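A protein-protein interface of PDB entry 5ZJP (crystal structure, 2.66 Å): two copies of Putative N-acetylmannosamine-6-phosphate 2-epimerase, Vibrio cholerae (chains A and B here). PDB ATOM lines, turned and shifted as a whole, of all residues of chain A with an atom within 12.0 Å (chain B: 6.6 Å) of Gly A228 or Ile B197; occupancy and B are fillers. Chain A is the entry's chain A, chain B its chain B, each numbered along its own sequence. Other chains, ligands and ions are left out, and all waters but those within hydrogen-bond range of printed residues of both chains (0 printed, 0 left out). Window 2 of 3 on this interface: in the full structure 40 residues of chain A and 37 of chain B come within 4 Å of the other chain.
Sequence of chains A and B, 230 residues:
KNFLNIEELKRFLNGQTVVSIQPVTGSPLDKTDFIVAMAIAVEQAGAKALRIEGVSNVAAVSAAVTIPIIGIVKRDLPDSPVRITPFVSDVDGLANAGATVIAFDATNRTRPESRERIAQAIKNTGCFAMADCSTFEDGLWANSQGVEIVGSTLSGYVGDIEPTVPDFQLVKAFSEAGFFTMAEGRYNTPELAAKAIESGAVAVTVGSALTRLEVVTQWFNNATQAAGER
Gly A228 touches just one residue of chain B: Ile B197 (3.9 Å).
No residue of chain A comes within 4 Å of Asn B14.
Of chain A, only Thr A224 (2.9 Å) and Gln A225 (3.1 Å) come within 4 Å of Gly B15.
No residue of chain A comes within 4 Å of Ala B196.
No residue of chain A comes within 4 Å of Glu B198.
No residue of chain A comes within 4 Å of Gly B200.
No residue of chain A comes within 4 Å of Val B202.
No residue of chain A comes within 4 Å of Ala B203.
Val B204 touches just one residue of chain A: Thr A224 (3.6 Å).
Printed residues of chain B within 4 Å of Ala A223: Ala B194 (3.7 Å).
Printed residues of chain A within 4 Å of Ala B194: Ala A223 (3.7 Å) and Ala A227 (3.98 Å).
Of the printed residues of chain A, Gln B16 touches Asn A221 (3.2 Å), Thr A224 (3.8 Å) and Gln A225 (2.9 Å).
Printed residues of chain B within 4 Å of Gln A225: Gly B15 and Gln B16.
Of the printed residues of chain B, Asn A221 touches Gln B16 (3.2 Å).
Phe A220 touches none of the printed residues of chain B.
Lys B195 touches none of the printed residues of chain A.
Of the 12 printed residues of chain A, 6 touch a printed residue of chain B.
Printed residues of chain A that touch a printed residue of chain B: Asn A221, Ala A223, Thr A224, Gln A225, Ala A227 and Gly A228.
Hydrophobic or aromatic side chains of chain A that line the printed part of chain B: Ala A227.
O of Asn A221 sits close to OG1 of Thr A224 (3.5 Å).
NE2 of Gln A225 sits at hydrogen-bond distance from O of Asn A221 (3.0 Å).
OG1 of Thr A224 lies within hydrogen-bond range of O of Phe A220 (3.2 Å).
The backbone NH (N) of Gly B15 is in hydrogen-bond range of the backbone carbonyl oxygen (O) of Val B202 (2.7 Å).
O of Gln B16 sits at hydrogen-bond distance from N of Val B204, at 3.2 Å.
No position is printed for both chains.
Among the printed residues, merely in contact across the chains: Ala A223 with Ala B194, Thr A224 with Gln B16, Thr A224 with Ala B193, Thr A224 with Ile B197, Thr A224 with Val B204, Ala A227 with Ala B194 and Gly A228 with Ile B197.
OG1 of Thr A224 is in hydrogen-bond range of O of Gly B15, 2.9 Å away.
The side-chain amide oxygen of Asn A221 sits close to the side-chain amide oxygen of Gln B16, at 3.2 Å.
OE1 of Gln A225 lies within hydrogen-bond range of NE2 of Gln B16 (2.9 Å).
The backbone NH (N) of Gln A225 sits at hydrogen-bond distance from the backbone carbonyl oxygen (O) of Gly B15, at 3.1 Å.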
ATOM      1  N   THR A 217     -20.583  -4.014 -35.406  1.00  0.00           N
ATOM      2  CA  THR A 217     -21.476  -3.422 -34.412  1.00  0.00           C
ATOM      3  C   THR A 217     -20.946  -3.640 -33.000  1.00  0.00           C
ATOM      4  O   THR A 217     -20.892  -2.707 -32.190  1.00  0.00           O
ATOM      5  CB  THR A 217     -22.885  -4.000 -34.554  1.00  0.00           C
ATOM      6  OG1 THR A 217     -23.485  -3.517 -35.762  1.00  0.00           O
ATOM      7  CG2 THR A 217     -23.752  -3.597 -33.370  1.00  0.00           C
ATOM      8  N   TRP A 219     -17.939  -4.140 -32.187  1.00  0.00           N
ATOM      9  CA  TRP A 219     -16.718  -3.352 -32.042  1.00  0.00           C
ATOM     10  C   TRP A 219     -17.012  -1.952 -31.514  1.00  0.00           C
ATOM     11  O   TRP A 219     -16.248  -1.414 -30.704  1.00  0.00           O
ATOM     12  CB  TRP A 219     -15.974  -3.290 -33.376  1.00  0.00           C
ATOM     13  CG  TRP A 219     -15.242  -4.555 -33.705  1.00  0.00           C
ATOM     14  CD1 TRP A 219     -15.039  -5.621 -32.876  1.00  0.00           C
ATOM     15  CD2 TRP A 219     -14.619  -4.891 -34.951  1.00  0.00           C
ATOM     16  NE1 TRP A 219     -14.325  -6.597 -33.527  1.00  0.00           N
ATOM     17  CE2 TRP A 219     -14.056  -6.175 -34.802  1.00  0.00           C
ATOM     18  CE3 TRP A 219     -14.484  -4.233 -36.176  1.00  0.00           C
ATOM     19  CZ2 TRP A 219     -13.367  -6.811 -35.833  1.00  0.00           C
ATOM     20  CZ3 TRP A 219     -13.798  -4.867 -37.198  1.00  0.00           C
ATOM     21  CH2 TRP A 219     -13.249  -6.142 -37.020  1.00  0.00           C
ATOM     22  N   PHE A 220     -18.114  -1.342 -31.960  1.00  0.00           N
ATOM     23  CA  PHE A 220     -18.446   0.006 -31.509  1.00  0.00           C
ATOM     24  C   PHE A 220     -19.060  -0.004 -30.114  1.00  0.00           C
ATOM     25  O   PHE A 220     -18.645   0.771 -29.245  1.00  0.00           O
ATOM     26  CB  PHE A 220     -19.386   0.694 -32.503  1.00  0.00           C
ATOM     27  CG  PHE A 220     -18.721   1.118 -33.786  1.00  0.00           C
ATOM     28  CD1 PHE A 220     -17.994   0.220 -34.550  1.00  0.00           C
ATOM     29  CD2 PHE A 220     -18.814   2.432 -34.216  1.00  0.00           C
ATOM     30  CE1 PHE A 220     -17.381   0.618 -35.721  1.00  0.00           C
ATOM     31  CE2 PHE A 220     -18.203   2.836 -35.387  1.00  0.00           C
ATOM     32  CZ  PHE A 220     -17.487   1.930 -36.140  1.00  0.00           C
ATOM     33  N   ASN A 221     -20.061  -0.860 -29.886  1.00  0.00           N
ATOM     34  CA  ASN A 221     -20.683  -0.927 -28.566  1.00  0.00           C
ATOM     35  C   ASN A 221     -19.666  -1.273 -27.485  1.00  0.00           C
ATOM     36  O   ASN A 221     -19.773  -0.781 -26.357  1.00  0.00           O
ATOM     37  CB  ASN A 221     -21.828  -1.941 -28.567  1.00  0.00           C
ATOM     38  CG  ASN A 221     -23.183  -1.293 -28.780  1.00  0.00           C
ATOM     39  OD1 ASN A 221     -23.368  -0.106 -28.510  1.00  0.00           O
ATOM     40  ND2 ASN A 221     -24.144  -2.075 -29.261  1.00  0.00           N
ATOM     41  N   ASN A 222     -18.678  -2.111 -27.805  1.00  0.00           N
ATOM     42  CA  ASN A 222     -17.618  -2.419 -26.848  1.00  0.00           C
ATOM     43  C   ASN A 222     -16.879  -1.158 -26.416  1.00  0.00           C
ATOM     44  O   ASN A 222     -16.525  -1.011 -25.242  1.00  0.00           O
ATOM     45  CB  ASN A 222     -16.637  -3.425 -27.449  1.00  0.00           C
ATOM     46  CG  ASN A 222     -17.077  -4.862 -27.247  1.00  0.00           C
ATOM     47  OD1 ASN A 222     -16.246  -5.765 -27.152  1.00  0.00           O
ATOM     48  ND2 ASN A 222     -18.383  -5.080 -27.167  1.00  0.00           N
ATOM     49  N   ALA A 223     -16.634  -0.239 -27.352  1.00  0.00           N
ATOM     50  CA  ALA A 223     -15.881   0.965 -27.021  1.00  0.00           C
ATOM     51  C   ALA A 223     -16.767   2.030 -26.387  1.00  0.00           C
ATOM     52  O   ALA A 223     -16.341   2.712 -25.449  1.00  0.00           O
ATOM     53  CB  ALA A 223     -15.197   1.516 -28.272  1.00  0.00           C
ATOM     54  N   THR A 224     -17.999   2.189 -26.879  1.00  0.00           N
ATOM     55  CA  THR A 224     -18.878   3.215 -26.328  1.00  0.00           C
ATOM     56  C   THR A 224     -19.435   2.819 -24.966  1.00  0.00           C
ATOM     57  O   THR A 224     -19.631   3.686 -24.107  1.00  0.00           O
ATOM     58  CB  THR A 224     -20.011   3.519 -27.307  1.00  0.00           C
ATOM     59  OG1 THR A 224     -20.815   2.348 -27.499  1.00  0.00           O
ATOM     60  CG2 THR A 224     -19.438   3.966 -28.640  1.00  0.00           C
ATOM     61  N   GLN A 225     -19.703   1.529 -24.750  1.00  0.00           N
ATOM     62  CA  GLN A 225     -20.195   1.097 -23.445  1.00  0.00           C
ATOM     63  C   GLN A 225     -19.085   1.129 -22.401  1.00  0.00           C
ATOM     64  O   GLN A 225     -19.321   1.509 -21.249  1.00  0.00           O
ATOM     65  CB  GLN A 225     -20.803  -0.302 -23.537  1.00  0.00           C
ATOM     66  CG  GLN A 225     -22.232  -0.335 -24.046  1.00  0.00           C
ATOM     67  CD  GLN A 225     -22.706  -1.743 -24.349  1.00  0.00           C
ATOM     68  OE1 GLN A 225     -23.753  -2.176 -23.865  1.00  0.00           O
ATOM     69  NE2 GLN A 225     -21.941  -2.464 -25.162  1.00  0.00           N
ATOM     70  N   ALA A 226     -17.873   0.715 -22.783  1.00  0.00           N
ATOM     71  CA  ALA A 226     -16.748   0.742 -21.854  1.00  0.00           C
ATOM     72  C   ALA A 226     -16.446   2.163 -21.396  1.00  0.00           C
ATOM     73  O   ALA A 226     -16.136   2.390 -20.221  1.00  0.00           O
ATOM     74  CB  ALA A 226     -15.513   0.115 -22.501  1.00  0.00           C
ATOM     75  N   ALA A 227     -16.521   3.129 -22.314  1.00  0.00           N
ATOM     76  CA  ALA A 227     -16.327   4.527 -21.946  1.00  0.00           C
ATOM     77  C   ALA A 227     -17.459   5.050 -21.071  1.00  0.00           C
ATOM     78  O   ALA A 227     -17.239   5.940 -20.243  1.00  0.00           O
ATOM     79  CB  ALA A 227     -16.190   5.386 -23.203  1.00  0.00           C
ATOM     80  N   GLY A 228     -18.666   4.516 -21.234  1.00  0.00           N
ATOM     81  CA  GLY A 228     -19.823   5.022 -20.522  1.00  0.00           C
ATOM     82  C   GLY A 228     -19.845   4.824 -19.018  1.00  0.00           C
ATOM     83  O   GLY A 228     -20.886   4.461 -18.462  1.00  0.00           O
ATOM     84  N   GLU A 229     -18.724   5.052 -18.341  1.00  0.00           N
ATOM     85  CA  GLU A 229     -18.720   5.036 -16.883  1.00  0.00           C
ATOM     86  C   GLU A 229     -18.646   6.467 -16.361  1.00  0.00           C
ATOM     87  O   GLU A 229     -19.647   7.038 -15.928  1.00  0.00           O
ATOM     88  CB  GLU A 229     -17.544   4.218 -16.345  1.00  0.00           C
ATOM     89  CG  GLU A 229     -17.473   2.799 -16.886  1.00  0.00           C
ATOM     90  CD  GLU A 229     -18.804   2.067 -16.891  1.00  0.00           C
ATOM     91  OE1 GLU A 229     -19.005   1.246 -17.810  1.00  0.00           O
ATOM     92  OE2 GLU A 229     -19.616   2.245 -15.958  1.00  0.00           O
ATOM     93  N   LEU B  13     -30.284   4.372 -23.389  1.00  0.00           N
ATOM     94  CA  LEU B  13     -29.343   4.713 -24.449  1.00  0.00           C
ATOM     95  C   LEU B  13     -27.954   5.085 -23.943  1.00  0.00           C
ATOM     96  O   LEU B  13     -27.080   5.380 -24.764  1.00  0.00           O
ATOM     97  CB  LEU B  13     -29.893   5.869 -25.290  1.00  0.00           C
ATOM     98  CG  LEU B  13     -31.160   5.606 -26.104  1.00  0.00           C
ATOM     99  CD1 LEU B  13     -31.544   6.845 -26.899  1.00  0.00           C
ATOM    100  CD2 LEU B  13     -30.973   4.408 -27.023  1.00  0.00           C
ATOM    101  N   ASN B  14     -27.727   5.088 -22.631  1.00  0.00           N
ATOM    102  CA  ASN B  14     -26.457   5.569 -22.099  1.00  0.00           C
ATOM    103  C   ASN B  14     -25.304   4.680 -22.552  1.00  0.00           C
ATOM    104  O   ASN B  14     -25.327   3.461 -22.358  1.00  0.00           O
ATOM    105  CB  ASN B  14     -26.506   5.629 -20.573  1.00  0.00           C
ATOM    106  CG  ASN B  14     -25.227   6.184 -19.974  1.00  0.00           C
ATOM    107  OD1 ASN B  14     -24.562   7.026 -20.576  1.00  0.00           O
ATOM    108  ND2 ASN B  14     -24.874   5.709 -18.785  1.00  0.00           N
ATOM    109  N   GLY B  15     -24.291   5.302 -23.152  1.00  0.00           N
ATOM    110  CA  GLY B  15     -23.127   4.582 -23.630  1.00  0.00           C
ATOM    111  C   GLY B  15     -23.354   3.696 -24.832  1.00  0.00           C
ATOM    112  O   GLY B  15     -22.472   2.902 -25.170  1.00  0.00           O
ATOM    113  N   GLN B  16     -24.506   3.798 -25.485  1.00  0.00           N
ATOM    114  CA  GLN B  16     -24.849   2.927 -26.598  1.00  0.00           C
ATOM    115  C   GLN B  16     -24.389   3.502 -27.935  1.00  0.00           C
ATOM    116  O   GLN B  16     -24.185   4.709 -28.093  1.00  0.00           O
ATOM    117  CB  GLN B  16     -26.356   2.672 -26.636  1.00  0.00           C
ATOM    118  CG  GLN B  16     -26.839   1.754 -25.534  1.00  0.00           C
ATOM    119  CD  GLN B  16     -26.198   0.383 -25.616  1.00  0.00           C
ATOM    120  OE1 GLN B  16     -26.047  -0.179 -26.702  1.00  0.00           O
ATOM    121  NE2 GLN B  16     -25.811  -0.160 -24.469  1.00  0.00           N
ATOM    122  N   PHE B 168     -15.967  17.288 -32.116  1.00  0.00           N
ATOM    123  CA  PHE B 168     -16.113  16.974 -30.702  1.00  0.00           C
ATOM    124  C   PHE B 168     -16.488  18.193 -29.873  1.00  0.00           C
ATOM    125  O   PHE B 168     -17.060  18.032 -28.790  1.00  0.00           O
ATOM    126  CB  PHE B 168     -14.825  16.353 -30.157  1.00  0.00           C
ATOM    127  CG  PHE B 168     -14.559  14.966 -30.665  1.00  0.00           C
ATOM    128  CD1 PHE B 168     -15.130  13.860 -30.053  1.00  0.00           C
ATOM    129  CD2 PHE B 168     -13.749  14.771 -31.766  1.00  0.00           C
ATOM    130  CE1 PHE B 168     -14.882  12.587 -30.527  1.00  0.00           C
ATOM    131  CE2 PHE B 168     -13.499  13.501 -32.249  1.00  0.00           C
ATOM    132  CZ  PHE B 168     -14.067  12.406 -31.625  1.00  0.00           C
ATOM    133  N   VAL B 171     -20.280  18.610 -29.429  1.00  0.00           N
ATOM    134  CA  VAL B 171     -20.768  17.582 -28.515  1.00  0.00           C
ATOM    135  C   VAL B 171     -20.453  17.964 -27.075  1.00  0.00           C
ATOM    136  O   VAL B 171     -21.280  17.783 -26.173  1.00  0.00           O
ATOM    137  CB  VAL B 171     -20.170  16.212 -28.885  1.00  0.00           C
ATOM    138  CG1 VAL B 171     -20.525  15.169 -27.837  1.00  0.00           C
ATOM    139  CG2 VAL B 171     -20.663  15.782 -30.254  1.00  0.00           C
ATOM    140  N   ALA B 183     -24.212  12.346 -30.151  1.00  0.00           N
ATOM    141  CA  ALA B 183     -23.103  12.601 -31.065  1.00  0.00           C
ATOM    142  C   ALA B 183     -23.340  11.847 -32.369  1.00  0.00           C
ATOM    143  O   ALA B 183     -23.490  10.621 -32.365  1.00  0.00           O
ATOM    144  CB  ALA B 183     -21.778  12.187 -30.431  1.00  0.00           C
ATOM    145  N   TYR B 187     -18.172   9.830 -37.054  1.00  0.00           N
ATOM    146  CA  TYR B 187     -17.579   8.968 -36.029  1.00  0.00           C
ATOM    147  C   TYR B 187     -17.361   7.595 -36.654  1.00  0.00           C
ATOM    148  O   TYR B 187     -18.194   6.694 -36.538  1.00  0.00           O
ATOM    149  CB  TYR B 187     -18.477   8.892 -34.802  1.00  0.00           C
ATOM    150  CG  TYR B 187     -18.595  10.194 -34.049  1.00  0.00           C
ATOM    151  CD1 TYR B 187     -17.611  10.592 -33.154  1.00  0.00           C
ATOM    152  CD2 TYR B 187     -19.682  11.033 -34.245  1.00  0.00           C
ATOM    153  CE1 TYR B 187     -17.716  11.781 -32.464  1.00  0.00           C
ATOM    154  CE2 TYR B 187     -19.794  12.228 -33.562  1.00  0.00           C
ATOM    155  CZ  TYR B 187     -18.805  12.596 -32.675  1.00  0.00           C
ATOM    156  OH  TYR B 187     -18.908  13.784 -31.993  1.00  0.00           O
ATOM    157  N   LEU B 192     -13.078   6.809 -31.924  1.00  0.00           N
ATOM    158  CA  LEU B 192     -13.624   8.155 -32.052  1.00  0.00           C
ATOM    159  C   LEU B 192     -15.056   8.222 -31.546  1.00  0.00           C
ATOM    160  O   LEU B 192     -15.498   9.281 -31.081  1.00  0.00           O
ATOM    161  CB  LEU B 192     -13.548   8.628 -33.510  1.00  0.00           C
ATOM    162  CG  LEU B 192     -12.127   8.944 -34.007  1.00  0.00           C
ATOM    163  CD1 LEU B 192     -11.959   8.718 -35.505  1.00  0.00           C
ATOM    164  CD2 LEU B 192     -11.797  10.360 -33.610  1.00  0.00           C
ATOM    165  N   ALA B 193     -15.806   7.124 -31.675  1.00  0.00           N
ATOM    166  CA  ALA B 193     -17.119   7.051 -31.056  1.00  0.00           C
ATOM    167  C   ALA B 193     -17.014   6.920 -29.543  1.00  0.00           C
ATOM    168  O   ALA B 193     -17.969   7.250 -28.833  1.00  0.00           O
ATOM    169  CB  ALA B 193     -17.909   5.881 -31.633  1.00  0.00           C
ATOM    170  N   ALA B 194     -15.874   6.435 -29.040  1.00  0.00           N
ATOM    171  CA  ALA B 194     -15.626   6.409 -27.605  1.00  0.00           C
ATOM    172  C   ALA B 194     -15.245   7.789 -27.086  1.00  0.00           C
ATOM    173  O   ALA B 194     -15.669   8.180 -25.993  1.00  0.00           O
ATOM    174  CB  ALA B 194     -14.536   5.388 -27.281  1.00  0.00           C
ATOM    175  N   LYS B 195     -14.440   8.533 -27.850  1.00  0.00           N
ATOM    176  CA  LYS B 195     -14.136   9.912 -27.483  1.00  0.00           C
ATOM    177  C   LYS B 195     -15.386  10.781 -27.453  1.00  0.00           C
ATOM    178  O   LYS B 195     -15.411  11.800 -26.754  1.00  0.00           O
ATOM    179  CB  LYS B 195     -13.095  10.500 -28.438  1.00  0.00           C
ATOM    180  CG  LYS B 195     -11.811   9.705 -28.484  1.00  0.00           C
ATOM    181  CD  LYS B 195     -11.290   9.534 -27.071  1.00  0.00           C
ATOM    182  CE  LYS B 195     -10.004   8.739 -27.014  1.00  0.00           C
ATOM    183  NZ  LYS B 195      -9.527   8.602 -25.609  1.00  0.00           N
ATOM    184  N   ALA B 196     -16.425  10.402 -28.199  1.00  0.00           N
ATOM    185  CA  ALA B 196     -17.684  11.139 -28.138  1.00  0.00           C
ATOM    186  C   ALA B 196     -18.350  10.960 -26.780  1.00  0.00           C
ATOM    187  O   ALA B 196     -18.803  11.932 -26.165  1.00  0.00           O
ATOM    188  CB  ALA B 196     -18.615  10.685 -29.260  1.00  0.00           C
ATOM    189  N   ILE B 197     -18.434   9.714 -26.305  1.00  0.00           N
ATOM    190  CA  ILE B 197     -18.991   9.456 -24.979  1.00  0.00           C
ATOM    191  C   ILE B 197     -18.168  10.170 -23.916  1.00  0.00           C
ATOM    192  O   ILE B 197     -18.717  10.767 -22.982  1.00  0.00           O
ATOM    193  CB  ILE B 197     -19.069   7.940 -24.718  1.00  0.00           C
ATOM    194  CG1 ILE B 197     -19.923   7.262 -25.789  1.00  0.00           C
ATOM    195  CG2 ILE B 197     -19.628   7.662 -23.329  1.00  0.00           C
ATOM    196  CD1 ILE B 197     -21.365   7.717 -25.798  1.00  0.00           C
ATOM    197  N   GLU B 198     -16.839  10.119 -24.040  1.00  0.00           N
ATOM    198  CA  GLU B 198     -15.984  10.837 -23.103  1.00  0.00           C
ATOM    199  C   GLU B 198     -16.160  12.344 -23.236  1.00  0.00           C
ATOM    200  O   GLU B 198     -15.933  13.081 -22.269  1.00  0.00           O
ATOM    201  CB  GLU B 198     -14.521  10.449 -23.321  1.00  0.00           C
ATOM    202  CG  GLU B 198     -14.234   8.972 -23.104  1.00  0.00           C
ATOM    203  CD  GLU B 198     -12.826   8.586 -23.509  1.00  0.00           C
ATOM    204  OE1 GLU B 198     -12.144   9.418 -24.139  1.00  0.00           O
ATOM    205  OE2 GLU B 198     -12.406   7.448 -23.211  1.00  0.00           O
ATOM    206  N   SER B 199     -16.554  12.819 -24.419  1.00  0.00           N
ATOM    207  CA  SER B 199     -16.909  14.220 -24.608  1.00  0.00           C
ATOM    208  C   SER B 199     -18.246  14.585 -23.976  1.00  0.00           C
ATOM    209  O   SER B 199     -18.617  15.764 -23.999  1.00  0.00           O
ATOM    210  CB  SER B 199     -16.939  14.557 -26.101  1.00  0.00           C
ATOM    211  OG  SER B 199     -15.632  14.580 -26.646  1.00  0.00           O
ATOM    212  N   GLY B 200     -18.976  13.619 -23.419  1.00  0.00           N
ATOM    213  CA  GLY B 200     -20.217  13.886 -22.717  1.00  0.00           C
ATOM    214  C   GLY B 200     -21.477  13.465 -23.441  1.00  0.00           C
ATOM    215  O   GLY B 200     -22.572  13.688 -22.913  1.00  0.00           O
ATOM    216  N   ALA B 201     -21.368  12.869 -24.626  1.00  0.00           N
ATOM    217  CA  ALA B 201     -22.546  12.382 -25.329  1.00  0.00           C
ATOM    218  C   ALA B 201     -23.180  11.216 -24.580  1.00  0.00           C
ATOM    219  O   ALA B 201     -22.487  10.348 -24.045  1.00  0.00           O
ATOM    220  CB  ALA B 201     -22.179  11.955 -26.750  1.00  0.00           C
ATOM    221  N   VAL B 202     -24.514  11.205 -24.539  1.00  0.00           N
ATOM    222  CA  VAL B 202     -25.227  10.085 -23.934  1.00  0.00           C
ATOM    223  C   VAL B 202     -25.082   8.839 -24.798  1.00  0.00           C
ATOM    224  O   VAL B 202     -24.747   7.754 -24.306  1.00  0.00           O
ATOM    225  CB  VAL B 202     -26.705  10.445 -23.712  1.00  0.00           C
ATOM    226  CG1 VAL B 202     -27.466   9.239 -23.186  1.00  0.00           C
ATOM    227  CG2 VAL B 202     -26.823  11.621 -22.757  1.00  0.00           C
ATOM    228  N   ALA B 203     -25.335   8.977 -26.097  1.00  0.00           N
ATOM    229  CA  ALA B 203     -25.151   7.903 -27.059  1.00  0.00           C
ATOM    230  C   ALA B 203     -24.462   8.482 -28.286  1.00  0.00           C
ATOM    231  O   ALA B 203     -24.145   9.674 -28.340  1.00  0.00           O
ATOM    232  CB  ALA B 203     -26.487   7.242 -27.423  1.00  0.00           C
ATOM    233  N   VAL B 204     -24.226   7.632 -29.280  1.00  0.00           N
ATOM    234  CA  VAL B 204     -23.559   8.044 -30.509  1.00  0.00           C
ATOM    235  C   VAL B 204     -24.176   7.291 -31.680  1.00  0.00           C
ATOM    236  O   VAL B 204     -24.434   6.086 -31.595  1.00  0.00           O
ATOM    237  CB  VAL B 204     -22.034   7.808 -30.431  1.00  0.00           C
ATOM    238  CG1 VAL B 204     -21.731   6.377 -30.024  1.00  0.00           C
ATOM    239  CG2 VAL B 204     -21.367   8.149 -31.758  1.00  0.00           C
